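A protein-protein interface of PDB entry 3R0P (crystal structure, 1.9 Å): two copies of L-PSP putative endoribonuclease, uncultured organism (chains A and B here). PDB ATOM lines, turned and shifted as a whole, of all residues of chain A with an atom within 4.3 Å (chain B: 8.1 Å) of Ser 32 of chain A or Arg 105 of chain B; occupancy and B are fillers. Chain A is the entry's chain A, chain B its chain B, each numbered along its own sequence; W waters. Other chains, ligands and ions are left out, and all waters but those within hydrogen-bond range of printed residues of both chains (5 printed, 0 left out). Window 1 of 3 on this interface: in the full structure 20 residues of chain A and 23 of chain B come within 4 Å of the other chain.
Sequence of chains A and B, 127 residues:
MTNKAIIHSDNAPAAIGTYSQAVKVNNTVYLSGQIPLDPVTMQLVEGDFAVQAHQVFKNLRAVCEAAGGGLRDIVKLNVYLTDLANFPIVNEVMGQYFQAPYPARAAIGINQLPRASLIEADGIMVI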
ATOM      1  N   ILE A  16     -14.530 -20.300   8.423  1.00  0.00           N
ATOM      2  CA  ILE A  16     -15.124 -19.025   8.035  1.00  0.00           C
ATOM      3  C   ILE A  16     -16.623 -19.045   8.317  1.00  0.00           C
ATOM      4  O   ILE A  16     -17.273 -20.077   8.173  1.00  0.00           O
ATOM      5  CB  ILE A  16     -14.911 -18.713   6.545  1.00  0.00           C
ATOM      6  CG1 ILE A  16     -15.604 -19.757   5.679  1.00  0.00           C
ATOM      7  CG2 ILE A  16     -13.426 -18.659   6.210  1.00  0.00           C
ATOM      8  CD1 ILE A  16     -15.777 -19.323   4.238  1.00  0.00           C
ATOM      9  N   THR A  18     -20.229 -18.911  10.420  1.00  0.00           N
ATOM     10  CA  THR A  18     -20.816 -19.122  11.736  1.00  0.00           C
ATOM     11  C   THR A  18     -20.570 -20.510  12.320  1.00  0.00           C
ATOM     12  O   THR A  18     -21.501 -21.166  12.799  1.00  0.00           O
ATOM     13  CB  THR A  18     -22.324 -18.812  11.743  1.00  0.00           C
ATOM     14  OG1 THR A  18     -22.965 -19.542  10.697  1.00  0.00           O
ATOM     15  CG2 THR A  18     -22.570 -17.303  11.543  1.00  0.00           C
ATOM     16  N   TYR A  19     -19.322 -20.964  12.287  1.00  0.00           N
ATOM     17  CA  TYR A  19     -18.982 -22.219  12.959  1.00  0.00           C
ATOM     18  C   TYR A  19     -17.562 -22.171  13.508  1.00  0.00           C
ATOM     19  O   TYR A  19     -16.794 -21.249  13.173  1.00  0.00           O
ATOM     20  CB  TYR A  19     -19.223 -23.436  12.047  1.00  0.00           C
ATOM     21  CG  TYR A  19     -18.100 -23.755  11.078  1.00  0.00           C
ATOM     22  CD1 TYR A  19     -17.337 -24.916  11.227  1.00  0.00           C
ATOM     23  CD2 TYR A  19     -17.822 -22.919  10.002  1.00  0.00           C
ATOM     24  CE1 TYR A  19     -16.322 -25.230  10.334  1.00  0.00           C
ATOM     25  CE2 TYR A  19     -16.810 -23.225   9.102  1.00  0.00           C
ATOM     26  CZ  TYR A  19     -16.063 -24.374   9.278  1.00  0.00           C
ATOM     27  OH  TYR A  19     -15.057 -24.665   8.395  1.00  0.00           O
ATOM     28  N   SER A  20     -17.242 -23.131  14.377  1.00  0.00           N
ATOM     29  CA  SER A  20     -15.901 -23.274  14.944  1.00  0.00           C
ATOM     30  C   SER A  20     -15.287 -24.557  14.397  1.00  0.00           C
ATOM     31  O   SER A  20     -16.006 -25.497  14.101  1.00  0.00           O
ATOM     32  CB  SER A  20     -15.969 -23.372  16.472  1.00  0.00           C
ATOM     33  OG  SER A  20     -16.572 -22.218  17.060  1.00  0.00           O
ATOM     34  N   GLN A  21     -13.966 -24.606  14.283  1.00  0.00           N
ATOM     35  CA  GLN A  21     -13.301 -25.833  13.846  1.00  0.00           C
ATOM     36  C   GLN A  21     -13.654 -26.978  14.782  1.00  0.00           C
ATOM     37  O   GLN A  21     -13.864 -28.109  14.350  1.00  0.00           O
ATOM     38  CB  GLN A  21     -11.783 -25.643  13.833  1.00  0.00           C
ATOM     39  CG  GLN A  21     -11.251 -24.843  12.659  1.00  0.00           C
ATOM     40  CD  GLN A  21      -9.746 -24.676  12.770  1.00  0.00           C
ATOM     41  OE1 GLN A  21      -9.201 -24.860  13.847  1.00  0.00           O
ATOM     42  NE2 GLN A  21      -9.073 -24.337  11.664  1.00  0.00           N
ATOM     43  N   TYR A  30     -15.988 -31.881  20.068  1.00  0.00           N
ATOM     44  CA  TYR A  30     -16.845 -32.010  18.898  1.00  0.00           C
ATOM     45  C   TYR A  30     -16.192 -31.387  17.670  1.00  0.00           C
ATOM     46  O   TYR A  30     -16.003 -30.169  17.604  1.00  0.00           O
ATOM     47  CB  TYR A  30     -18.209 -31.375  19.187  1.00  0.00           C
ATOM     48  CG  TYR A  30     -18.899 -32.118  20.307  1.00  0.00           C
ATOM     49  CD1 TYR A  30     -19.752 -33.171  20.027  1.00  0.00           C
ATOM     50  CD2 TYR A  30     -18.629 -31.830  21.642  1.00  0.00           C
ATOM     51  CE1 TYR A  30     -20.360 -33.881  21.026  1.00  0.00           C
ATOM     52  CE2 TYR A  30     -19.254 -32.563  22.667  1.00  0.00           C
ATOM     53  CZ  TYR A  30     -20.111 -33.574  22.343  1.00  0.00           C
ATOM     54  OH  TYR A  30     -20.740 -34.315  23.331  1.00  0.00           O
ATOM     55  N   LEU A  31     -15.863 -32.228  16.692  1.00  0.00           N
ATOM     56  CA  LEU A  31     -15.112 -31.787  15.519  1.00  0.00           C
ATOM     57  C   LEU A  31     -16.033 -31.462  14.354  1.00  0.00           C
ATOM     58  O   LEU A  31     -16.887 -32.269  13.998  1.00  0.00           O
ATOM     59  CB  LEU A  31     -14.137 -32.892  15.082  1.00  0.00           C
ATOM     60  CG  LEU A  31     -13.127 -33.345  16.136  1.00  0.00           C
ATOM     61  CD1 LEU A  31     -12.633 -34.770  15.840  1.00  0.00           C
ATOM     62  CD2 LEU A  31     -11.960 -32.364  16.197  1.00  0.00           C
ATOM     63  N   SER A  32     -15.844 -30.294  13.745  1.00  0.00           N
ATOM     64  CA  SER A  32     -16.541 -29.973  12.504  1.00  0.00           C
ATOM     65  C   SER A  32     -16.098 -30.852  11.347  1.00  0.00           C
ATOM     66  O   SER A  32     -15.012 -31.425  11.368  1.00  0.00           O
ATOM     67  CB  SER A  32     -16.288 -28.512  12.126  1.00  0.00           C
ATOM     68  OG  SER A  32     -16.824 -27.665  13.120  1.00  0.00           O
ATOM     69  N   GLY A  33     -16.930 -30.922  10.318  1.00  0.00           N
ATOM     70  CA  GLY A  33     -16.564 -31.606   9.097  1.00  0.00           C
ATOM     71  C   GLY A  33     -15.364 -30.964   8.426  1.00  0.00           C
ATOM     72  O   GLY A  33     -15.324 -29.750   8.244  1.00  0.00           O
ATOM     73  N   GLN A  34     -14.380 -31.779   8.060  1.00  0.00           N
ATOM     74  CA  GLN A  34     -13.226 -31.295   7.305  1.00  0.00           C
ATOM     75  C   GLN A  34     -13.327 -31.834   5.890  1.00  0.00           C
ATOM     76  O   GLN A  34     -13.696 -32.992   5.688  1.00  0.00           O
ATOM     77  CB  GLN A  34     -11.914 -31.773   7.933  1.00  0.00           C
ATOM     78  CG  GLN A  34     -11.613 -31.122   9.249  1.00  0.00           C
ATOM     79  CD  GLN A  34     -11.356 -29.622   9.077  1.00  0.00           C
ATOM     80  OE1 GLN A  34     -10.770 -29.197   8.086  1.00  0.00           O
ATOM     81  NE2 GLN A  34     -11.822 -28.827  10.021  1.00  0.00           N
ATOM     82  N   LEU A  60      -8.060 -32.971  10.062  1.00  0.00           N
ATOM     83  CA  LEU A  60      -8.635 -33.384  11.333  1.00  0.00           C
ATOM     84  C   LEU A  60      -7.558 -33.496  12.395  1.00  0.00           C
ATOM     85  O   LEU A  60      -7.755 -33.065  13.538  1.00  0.00           O
ATOM     86  CB  LEU A  60      -9.361 -34.736  11.210  1.00  0.00           C
ATOM     87  CG  LEU A  60     -10.771 -34.701  10.633  1.00  0.00           C
ATOM     88  CD1 LEU A  60     -11.264 -36.143  10.377  1.00  0.00           C
ATOM     89  CD2 LEU A  60     -11.723 -33.922  11.568  1.00  0.00           C
ATOM     90  N   ALA A 121     -15.143 -35.598   6.525  1.00  0.00           N
ATOM     91  CA  ALA A 121     -15.266 -36.424   7.723  1.00  0.00           C
ATOM     92  C   ALA A 121     -15.371 -35.542   8.946  1.00  0.00           C
ATOM     93  O   ALA A 121     -14.710 -34.506   9.041  1.00  0.00           O
ATOM     94  CB  ALA A 121     -14.084 -37.376   7.852  1.00  0.00           C
ATOM     95  N   ASP A 122     -16.234 -35.917   9.878  1.00  0.00           N
ATOM     96  CA  ASP A 122     -16.307 -35.166  11.133  1.00  0.00           C
ATOM     97  C   ASP A 122     -16.295 -36.178  12.264  1.00  0.00           C
ATOM     98  O   ASP A 122     -16.174 -37.369  12.016  1.00  0.00           O
ATOM     99  CB  ASP A 122     -17.538 -34.251  11.180  1.00  0.00           C
ATOM    100  CG  ASP A 122     -18.832 -35.014  11.322  1.00  0.00           C
ATOM    101  OD1 ASP A 122     -18.844 -36.219  11.052  1.00  0.00           O
ATOM    102  OD2 ASP A 122     -19.845 -34.408  11.704  1.00  0.00           O
ATOM    103  N   PHE B  57     -34.323 -23.359  12.934  1.00  0.00           N
ATOM    104  CA  PHE B  57     -33.651 -22.846  14.120  1.00  0.00           C
ATOM    105  C   PHE B  57     -34.596 -22.440  15.252  1.00  0.00           C
ATOM    106  O   PHE B  57     -34.284 -22.643  16.431  1.00  0.00           O
ATOM    107  CB  PHE B  57     -32.640 -21.768  13.736  1.00  0.00           C
ATOM    108  CG  PHE B  57     -31.533 -22.308  12.870  1.00  0.00           C
ATOM    109  CD1 PHE B  57     -30.690 -23.292  13.361  1.00  0.00           C
ATOM    110  CD2 PHE B  57     -31.385 -21.896  11.560  1.00  0.00           C
ATOM    111  CE1 PHE B  57     -29.689 -23.828  12.568  1.00  0.00           C
ATOM    112  CE2 PHE B  57     -30.382 -22.425  10.762  1.00  0.00           C
ATOM    113  CZ  PHE B  57     -29.536 -23.389  11.267  1.00  0.00           C
ATOM    114  N   ILE B  74     -25.531 -25.264  22.087  1.00  0.00           N
ATOM    115  CA  ILE B  74     -25.267 -26.271  21.065  1.00  0.00           C
ATOM    116  C   ILE B  74     -23.766 -26.322  20.810  1.00  0.00           C
ATOM    117  O   ILE B  74     -23.124 -25.282  20.603  1.00  0.00           O
ATOM    118  CB  ILE B  74     -26.047 -25.964  19.775  1.00  0.00           C
ATOM    119  CG1 ILE B  74     -27.549 -26.195  20.022  1.00  0.00           C
ATOM    120  CG2 ILE B  74     -25.554 -26.823  18.622  1.00  0.00           C
ATOM    121  CD1 ILE B  74     -28.427 -25.967  18.822  1.00  0.00           C
ATOM    122  N   VAL B  75     -23.195 -27.524  20.865  1.00  0.00           N
ATOM    123  CA  VAL B  75     -21.760 -27.698  20.631  1.00  0.00           C
ATOM    124  C   VAL B  75     -21.463 -28.243  19.234  1.00  0.00           C
ATOM    125  O   VAL B  75     -20.381 -28.032  18.684  1.00  0.00           O
ATOM    126  CB  VAL B  75     -21.119 -28.636  21.685  1.00  0.00           C
ATOM    127  CG1 VAL B  75     -21.161 -27.986  23.074  1.00  0.00           C
ATOM    128  CG2 VAL B  75     -21.800 -30.029  21.688  1.00  0.00           C
ATOM    129  N   LYS B  76     -22.425 -28.962  18.673  1.00  0.00           N
ATOM    130  CA  LYS B  76     -22.275 -29.506  17.342  1.00  0.00           C
ATOM    131  C   LYS B  76     -23.602 -29.452  16.615  1.00  0.00           C
ATOM    132  O   LYS B  76     -24.625 -29.884  17.132  1.00  0.00           O
ATOM    133  CB  LYS B  76     -21.799 -30.969  17.412  1.00  0.00           C
ATOM    134  CG  LYS B  76     -21.768 -31.677  16.061  1.00  0.00           C
ATOM    135  CD  LYS B  76     -20.745 -31.039  15.135  1.00  0.00           C
ATOM    136  CE  LYS B  76     -20.657 -31.766  13.791  1.00  0.00           C
ATOM    137  NZ  LYS B  76     -20.345 -33.217  13.950  1.00  0.00           N
ATOM    138  N   LEU B  77     -23.566 -28.974  15.385  1.00  0.00           N
ATOM    139  CA  LEU B  77     -24.763 -28.892  14.575  1.00  0.00           C
ATOM    140  C   LEU B  77     -24.521 -29.628  13.263  1.00  0.00           C
ATOM    141  O   LEU B  77     -23.504 -29.408  12.597  1.00  0.00           O
ATOM    142  CB  LEU B  77     -25.061 -27.412  14.302  1.00  0.00           C
ATOM    143  CG  LEU B  77     -26.399 -27.041  13.686  1.00  0.00           C
ATOM    144  CD1 LEU B  77     -27.504 -27.238  14.709  1.00  0.00           C
ATOM    145  CD2 LEU B  77     -26.350 -25.590  13.211  1.00  0.00           C
ATOM    146  N   ASN B  78     -25.439 -30.515  12.896  1.00  0.00           N
ATOM    147  CA  ASN B  78     -25.409 -31.152  11.584  1.00  0.00           C
ATOM    148  C   ASN B  78     -26.495 -30.536  10.716  1.00  0.00           C
ATOM    149  O   ASN B  78     -27.669 -30.511  11.102  1.00  0.00           O
ATOM    150  CB  ASN B  78     -25.647 -32.663  11.694  1.00  0.00           C
ATOM    151  CG  ASN B  78     -24.619 -33.353  12.571  1.00  0.00           C
ATOM    152  OD1 ASN B  78     -24.964 -33.993  13.570  1.00  0.00           O
ATOM    153  ND2 ASN B  78     -23.353 -33.218  12.211  1.00  0.00           N
ATOM    154  N   VAL B  79     -26.110 -30.043   9.549  1.00  0.00           N
ATOM    155  CA  VAL B  79     -27.059 -29.407   8.646  1.00  0.00           C
ATOM    156  C   VAL B  79     -27.152 -30.211   7.357  1.00  0.00           C
ATOM    157  O   VAL B  79     -26.157 -30.369   6.646  1.00  0.00           O
ATOM    158  CB  VAL B  79     -26.640 -27.961   8.321  1.00  0.00           C
ATOM    159  CG1 VAL B  79     -27.600 -27.341   7.310  1.00  0.00           C
ATOM    160  CG2 VAL B  79     -26.586 -27.123   9.603  1.00  0.00           C
ATOM    161  N   PHE B  87     -26.432 -23.259   1.086  1.00  0.00           N
ATOM    162  CA  PHE B  87     -25.701 -23.146   2.337  1.00  0.00           C
ATOM    163  C   PHE B  87     -25.327 -21.719   2.784  1.00  0.00           C
ATOM    164  O   PHE B  87     -25.370 -21.429   3.979  1.00  0.00           O
ATOM    165  CB  PHE B  87     -24.492 -24.077   2.404  1.00  0.00           C
ATOM    166  CG  PHE B  87     -23.955 -24.214   3.783  1.00  0.00           C
ATOM    167  CD1 PHE B  87     -24.668 -24.917   4.741  1.00  0.00           C
ATOM    168  CD2 PHE B  87     -22.779 -23.592   4.147  1.00  0.00           C
ATOM    169  CE1 PHE B  87     -24.202 -25.022   6.031  1.00  0.00           C
ATOM    170  CE2 PHE B  87     -22.303 -23.695   5.434  1.00  0.00           C
ATOM    171  CZ  PHE B  87     -23.015 -24.411   6.378  1.00  0.00           C
ATOM    172  N   PRO B  88     -24.962 -20.829   1.842  1.00  0.00           N
ATOM    173  CA  PRO B  88     -24.639 -19.471   2.292  1.00  0.00           C
ATOM    174  C   PRO B  88     -25.810 -18.833   3.035  1.00  0.00           C
ATOM    175  O   PRO B  88     -25.596 -18.035   3.947  1.00  0.00           O
ATOM    176  CB  PRO B  88     -24.359 -18.724   0.984  1.00  0.00           C
ATOM    177  CG  PRO B  88     -23.893 -19.780   0.053  1.00  0.00           C
ATOM    178  CD  PRO B  88     -24.679 -21.016   0.409  1.00  0.00           C
ATOM    179  N   VAL B  90     -27.991 -20.522   4.938  1.00  0.00           N
ATOM    180  CA  VAL B  90     -27.955 -21.139   6.262  1.00  0.00           C
ATOM    181  C   VAL B  90     -26.912 -20.439   7.119  1.00  0.00           C
ATOM    182  O   VAL B  90     -27.158 -20.081   8.272  1.00  0.00           O
ATOM    183  CB  VAL B  90     -27.598 -22.647   6.197  1.00  0.00           C
ATOM    184  CG1 VAL B  90     -27.521 -23.235   7.595  1.00  0.00           C
ATOM    185  CG2 VAL B  90     -28.614 -23.409   5.366  1.00  0.00           C
ATOM    186  N   ASN B  91     -25.733 -20.245   6.541  1.00  0.00           N
ATOM    187  CA  ASN B  91     -24.651 -19.604   7.255  1.00  0.00           C
ATOM    188  C   ASN B  91     -25.064 -18.229   7.769  1.00  0.00           C
ATOM    189  O   ASN B  91     -24.756 -17.849   8.902  1.00  0.00           O
ATOM    190  CB  ASN B  91     -23.423 -19.499   6.357  1.00  0.00           C
ATOM    191  CG  ASN B  91     -22.253 -18.881   7.063  1.00  0.00           C
ATOM    192  OD1 ASN B  91     -21.548 -19.547   7.819  1.00  0.00           O
ATOM    193  ND2 ASN B  91     -22.051 -17.591   6.845  1.00  0.00           N
ATOM    194  N   GLU B  92     -25.790 -17.495   6.939  1.00  0.00           N
ATOM    195  CA  GLU B  92     -26.173 -16.134   7.266  1.00  0.00           C
ATOM    196  C   GLU B  92     -27.337 -16.075   8.250  1.00  0.00           C
ATOM    197  O   GLU B  92     -27.336 -15.262   9.175  1.00  0.00           O
ATOM    198  CB  GLU B  92     -26.519 -15.369   5.993  1.00  0.00           C
ATOM    199  CG  GLU B  92     -26.824 -13.897   6.227  1.00  0.00           C
ATOM    200  CD  GLU B  92     -26.967 -13.131   4.930  1.00  0.00           C
ATOM    201  OE1 GLU B  92     -26.865 -13.760   3.853  1.00  0.00           O
ATOM    202  OE2 GLU B  92     -27.176 -11.904   4.988  1.00  0.00           O
ATOM    203  N   VAL B  93     -28.332 -16.932   8.047  1.00  0.00           N
ATOM    204  CA  VAL B  93     -29.458 -17.017   8.972  1.00  0.00           C
ATOM    205  C   VAL B  93     -28.966 -17.391  10.361  1.00  0.00           C
ATOM    206  O   VAL B  93     -29.469 -16.881  11.356  1.00  0.00           O
ATOM    207  CB  VAL B  93     -30.494 -18.059   8.516  1.00  0.00           C
ATOM    208  CG1 VAL B  93     -31.480 -18.361   9.635  1.00  0.00           C
ATOM    209  CG2 VAL B  93     -31.208 -17.581   7.256  1.00  0.00           C
ATOM    210  N   MET B  94     -27.971 -18.277  10.422  1.00  0.00           N
ATOM    211  CA  MET B  94     -27.423 -18.707  11.704  1.00  0.00           C
ATOM    212  C   MET B  94     -26.911 -17.528  12.514  1.00  0.00           C
ATOM    213  O   MET B  94     -26.946 -17.549  13.745  1.00  0.00           O
ATOM    214  CB  MET B  94     -26.331 -19.794  11.522  1.00  0.00           C
ATOM    215  CG  MET B  94     -26.913 -21.191  11.323  1.00  0.00           C
ATOM    216  SD  MET B  94     -25.737 -22.583  11.432  1.00  0.00           S
ATOM    217  CE  MET B  94     -24.904 -22.196  12.967  1.00  0.00           C
ATOM    218  N   GLY B  95     -26.457 -16.487  11.815  1.00  0.00           N
ATOM    219  CA  GLY B  95     -25.948 -15.298  12.464  1.00  0.00           C
ATOM    220  C   GLY B  95     -26.999 -14.574  13.297  1.00  0.00           C
ATOM    221  O   GLY B  95     -26.652 -13.815  14.202  1.00  0.00           O
ATOM    222  N   PHE B  98     -27.364 -17.434  16.528  1.00  0.00           N
ATOM    223  CA  PHE B  98     -26.159 -17.789  17.252  1.00  0.00           C
ATOM    224  C   PHE B  98     -25.211 -16.596  17.293  1.00  0.00           C
ATOM    225  O   PHE B  98     -25.169 -15.789  16.367  1.00  0.00           O
ATOM    226  CB  PHE B  98     -25.432 -18.954  16.544  1.00  0.00           C
ATOM    227  CG  PHE B  98     -26.213 -20.240  16.480  1.00  0.00           C
ATOM    228  CD1 PHE B  98     -25.948 -21.274  17.371  1.00  0.00           C
ATOM    229  CD2 PHE B  98     -27.178 -20.440  15.505  1.00  0.00           C
ATOM    230  CE1 PHE B  98     -26.655 -22.472  17.306  1.00  0.00           C
ATOM    231  CE2 PHE B  98     -27.887 -21.643  15.434  1.00  0.00           C
ATOM    232  CZ  PHE B  98     -27.623 -22.654  16.338  1.00  0.00           C
ATOM    233  N   TYR B 102     -19.345 -20.007  18.031  1.00  0.00           N
ATOM    234  CA  TYR B 102     -20.282 -20.853  17.298  1.00  0.00           C
ATOM    235  C   TYR B 102     -20.041 -22.351  17.536  1.00  0.00           C
ATOM    236  O   TYR B 102     -18.952 -22.752  17.927  1.00  0.00           O
ATOM    237  CB  TYR B 102     -20.175 -20.553  15.805  1.00  0.00           C
ATOM    238  CG  TYR B 102     -20.422 -19.099  15.477  1.00  0.00           C
ATOM    239  CD1 TYR B 102     -21.710 -18.583  15.494  1.00  0.00           C
ATOM    240  CD2 TYR B 102     -19.370 -18.243  15.147  1.00  0.00           C
ATOM    241  CE1 TYR B 102     -21.955 -17.251  15.198  1.00  0.00           C
ATOM    242  CE2 TYR B 102     -19.604 -16.901  14.841  1.00  0.00           C
ATOM    243  CZ  TYR B 102     -20.903 -16.414  14.873  1.00  0.00           C
ATOM    244  OH  TYR B 102     -21.168 -15.093  14.580  1.00  0.00           O
ATOM    245  N   PRO B 103     -21.069 -23.173  17.308  1.00  0.00           N
ATOM    246  CA  PRO B 103     -20.913 -24.627  17.456  1.00  0.00           C
ATOM    247  C   PRO B 103     -20.021 -25.177  16.352  1.00  0.00           C
ATOM    248  O   PRO B 103     -19.805 -24.501  15.337  1.00  0.00           O
ATOM    249  CB  PRO B 103     -22.337 -25.155  17.286  1.00  0.00           C
ATOM    250  CG  PRO B 103     -23.074 -24.100  16.550  1.00  0.00           C
ATOM    251  CD  PRO B 103     -22.455 -22.790  16.984  1.00  0.00           C
ATOM    252  N   ALA B 104     -19.492 -26.378  16.555  1.00  0.00           N
ATOM    253  CA  ALA B 104     -18.895 -27.107  15.454  1.00  0.00           C
ATOM    254  C   ALA B 104     -20.032 -27.408  14.485  1.00  0.00           C
ATOM    255  O   ALA B 104     -21.200 -27.365  14.867  1.00  0.00           O
ATOM    256  CB  ALA B 104     -18.264 -28.394  15.952  1.00  0.00           C
ATOM    257  N   ARG B 105     -19.710 -27.679  13.229  1.00  0.00           N
ATOM    258  CA  ARG B 105     -20.752 -27.853  12.223  1.00  0.00           C
ATOM    259  C   ARG B 105     -20.315 -28.802  11.117  1.00  0.00           C
ATOM    260  O   ARG B 105     -19.137 -28.862  10.756  1.00  0.00           O
ATOM    261  CB  ARG B 105     -21.103 -26.491  11.614  1.00  0.00           C
ATOM    262  CG  ARG B 105     -22.307 -26.486  10.676  1.00  0.00           C
ATOM    263  CD  ARG B 105     -22.732 -25.044  10.325  1.00  0.00           C
ATOM    264  NE  ARG B 105     -21.740 -24.308   9.530  1.00  0.00           N
ATOM    265  CZ  ARG B 105     -21.770 -22.989   9.336  1.00  0.00           C
ATOM    266  NH1 ARG B 105     -22.720 -22.257   9.901  1.00  0.00           N
ATOM    267  NH2 ARG B 105     -20.843 -22.394   8.594  1.00  0.00           N
ATOM    268  N   ALA B 106     -21.264 -29.553  10.584  1.00  0.00           N
ATOM    269  CA  ALA B 106     -21.033 -30.317   9.371  1.00  0.00           C
ATOM    270  C   ALA B 106     -22.194 -30.044   8.436  1.00  0.00           C
ATOM    271  O   ALA B 106     -23.345 -30.034   8.862  1.00  0.00           O
ATOM    272  CB  ALA B 106     -20.913 -31.799   9.678  1.00  0.00           C
ATOM    273  N   ALA B 107     -21.891 -29.775   7.174  1.00  0.00           N
ATOM    274  CA  ALA B 107     -22.921 -29.474   6.190  1.00  0.00           C
ATOM    275  C   ALA B 107     -22.819 -30.462   5.043  1.00  0.00           C
ATOM    276  O   ALA B 107     -21.769 -30.592   4.414  1.00  0.00           O
ATOM    277  CB  ALA B 107     -22.778 -28.061   5.679  1.00  0.00           C
ATOM    278  N   ILE B 108     -23.913 -31.167   4.779  1.00  0.00           N
ATOM    279  CA  ILE B 108     -23.883 -32.252   3.815  1.00  0.00           C
ATOM    280  C   ILE B 108     -25.011 -32.105   2.806  1.00  0.00           C
ATOM    281  O   ILE B 108     -26.146 -31.800   3.181  1.00  0.00           O
ATOM    282  CB  ILE B 108     -24.094 -33.606   4.527  1.00  0.00           C
ATOM    283  CG1 ILE B 108     -23.241 -33.685   5.794  1.00  0.00           C
ATOM    284  CG2 ILE B 108     -23.794 -34.753   3.582  1.00  0.00           C
ATOM    285  CD1 ILE B 108     -21.749 -33.623   5.514  1.00  0.00           C
ATOM    286  N   ASP B 122     -29.820 -31.266  13.043  1.00  0.00           N
ATOM    287  CA  ASP B 122     -29.835 -31.873  14.362  1.00  0.00           C
ATOM    288  C   ASP B 122     -28.543 -31.504  15.066  1.00  0.00           C
ATOM    289  O   ASP B 122     -27.721 -30.742  14.527  1.00  0.00           O
ATOM    290  CB  ASP B 122     -30.062 -33.394  14.289  1.00  0.00           C
ATOM    291  CG  ASP B 122     -28.813 -34.173  13.879  1.00  0.00           C
ATOM    292  OD1 ASP B 122     -27.845 -33.577  13.370  1.00  0.00           O
ATOM    293  OD2 ASP B 122     -28.812 -35.405  14.060  1.00  0.00           O
HETATM  294  O   HOH W   1     -19.066 -33.797  15.987  1.00  0.00           O
HETATM  295  O   HOH W   2     -22.190 -23.931  13.615  1.00  0.00           O
HETATM  296  O   HOH W   3     -21.963 -35.335  11.030  1.00  0.00           O
HETATM  297  O   HOH W   4     -17.796 -27.731   8.310  1.00  0.00           O
HETATM  298  O   HOH W   5     -16.804 -19.438  16.947  1.00  0.00           O
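The backbone NH of Thr 18 of chain A is in hydrogen-bond range of the side-chain amide oxygen of Asn 91 of chain B, at 3.0 Å. OG1 of Thr 18 of chain A is in hydrogen-bond range of NH1 of Arg 105 of chain B. O of Tyr 102 of chain B lies within hydrogen-bond range of OG of Ser 20 of chain A, at 2.6 Å. The backbone NH (N) of Ser 20 of chain A is in hydrogen-bond range of the backbone carbonyl oxygen (O) of Pro 103 of chain B (3.1 Å). N of Arg 105 of chain B sits at hydrogen-bond distance from OG of Ser 32 of chain A, 2.9 Å away. N of Gly 33 of chain A is in hydrogen-bond range of O of Arg 105 of chain B, 3.1 Å away. The side-chain carboxylate (OD2) of Asp 122 of chain A lies within salt-bridge range of the side-chain amino group (NZ) of Lys 76 of chain B (2.6 Å).
The backbone carbonyl oxygen (O) of Gln 21 of chain A is in hydrogen-bond range of the backbone NH (N) of Ser 32 of chain A. O of Val 75 of chain B sits at hydrogen-bond distance from N of Ala 104 of chain B. N of Ala 106 of chain B lies within hydrogen-bond range of O of Leu 77 of chain B (3.0 Å). The guanidinium group of Arg 105 of chain B sits at hydrogen-bond distance from the side-chain sulfur of Met 94 of chain B, 3.4 Å away.
Among the printed residues, pairs that only touch across the chains: Ser 32 of chain A with Ala 104 of chain B, Tyr 30 of chain A with Ala 104 of chain B, Thr 18 of chain A with Tyr 102 of chain B, Tyr 19 of chain A with Arg 105 of chain B, Tyr 19 of chain A with Pro 103 of chain B, Asp 122 of chain A with Ala 106 of chain B, Thr 18 of chain A with Met 94 of chain B, Tyr 19 of chain A with Tyr 102 of chain B, Ser 20 of chain A with Ala 104 of chain B, Leu 31 of chain A with Lys 76 of chain B, Tyr 30 of chain A with Val 75 of chain B, Asp 122 of chain A with Asn 78 of chain B, Thr 18 of chain A with Gly 95 of chain B and Tyr 30 of chain A with Lys 76 of chain B.
Printed residues of chain B within 4 Å of Tyr 19 of chain A: Tyr 102, Pro 103 and Arg 105. Printed residues of chain B within 4 Å of Leu 31 of chain A: Lys 76 (3.6 Å). Of the printed residues of chain B, Asp 122 of chain A touches Lys 76 (2.6 Å), Asn 78 (3.7 Å) and Ala 106 (3.5 Å). Val 79 of chain B touches none of the printed residues of chain A. Of the printed residues of chain A, Tyr 102 of chain B touches Thr 18, Tyr 19 and Ser 20. Arg 105 of chain B touches just these residues of chain A: Thr 18, Tyr 19, Ser 32 and Gly 33. Ile 108 of chain B touches none of the printed residues of chain A. The nearest printed residue of chain A that does not touch Arg 105 of chain B is Ile 16 of chain A (4.3 Å). The nearest printed residue of chain A that does not touch Tyr 102 of chain B is Gln 21 of chain A (6.4 Å).
Printed residues of chain A that touch a printed residue of chain B: Thr 18, Tyr 19, Ser 20, Tyr 30, Leu 31, Ser 32, Gly 33 and Asp 122. Hydrophobic or aromatic side chains of chain A that line the printed part of chain B: Tyr 19 and Tyr 30. Of the 24 printed residues of chain B, 11 touch a printed residue of chain A. Hydrophobic or aromatic side chains of chain B that line the printed part of chain A: Val 75, Met 94, Tyr 102, Ala 104 and Ala 106.
Position printed for both chains: 122.
Water W3 bridges the side-chain carboxylate of Asp 122 of chain A and the side-chain amide nitrogen of Asn 78 of chain B. Water W5 lies within hydrogen-bond range of the side-chain hydroxyl of Ser 20 of chain A (2.8 Å) and the backbone NH of Tyr 102 of chain B (2.8 Å). Water W4 lies within hydrogen-bond range of O of Arg 105 of chain B and O of Gly 33 of chain A.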
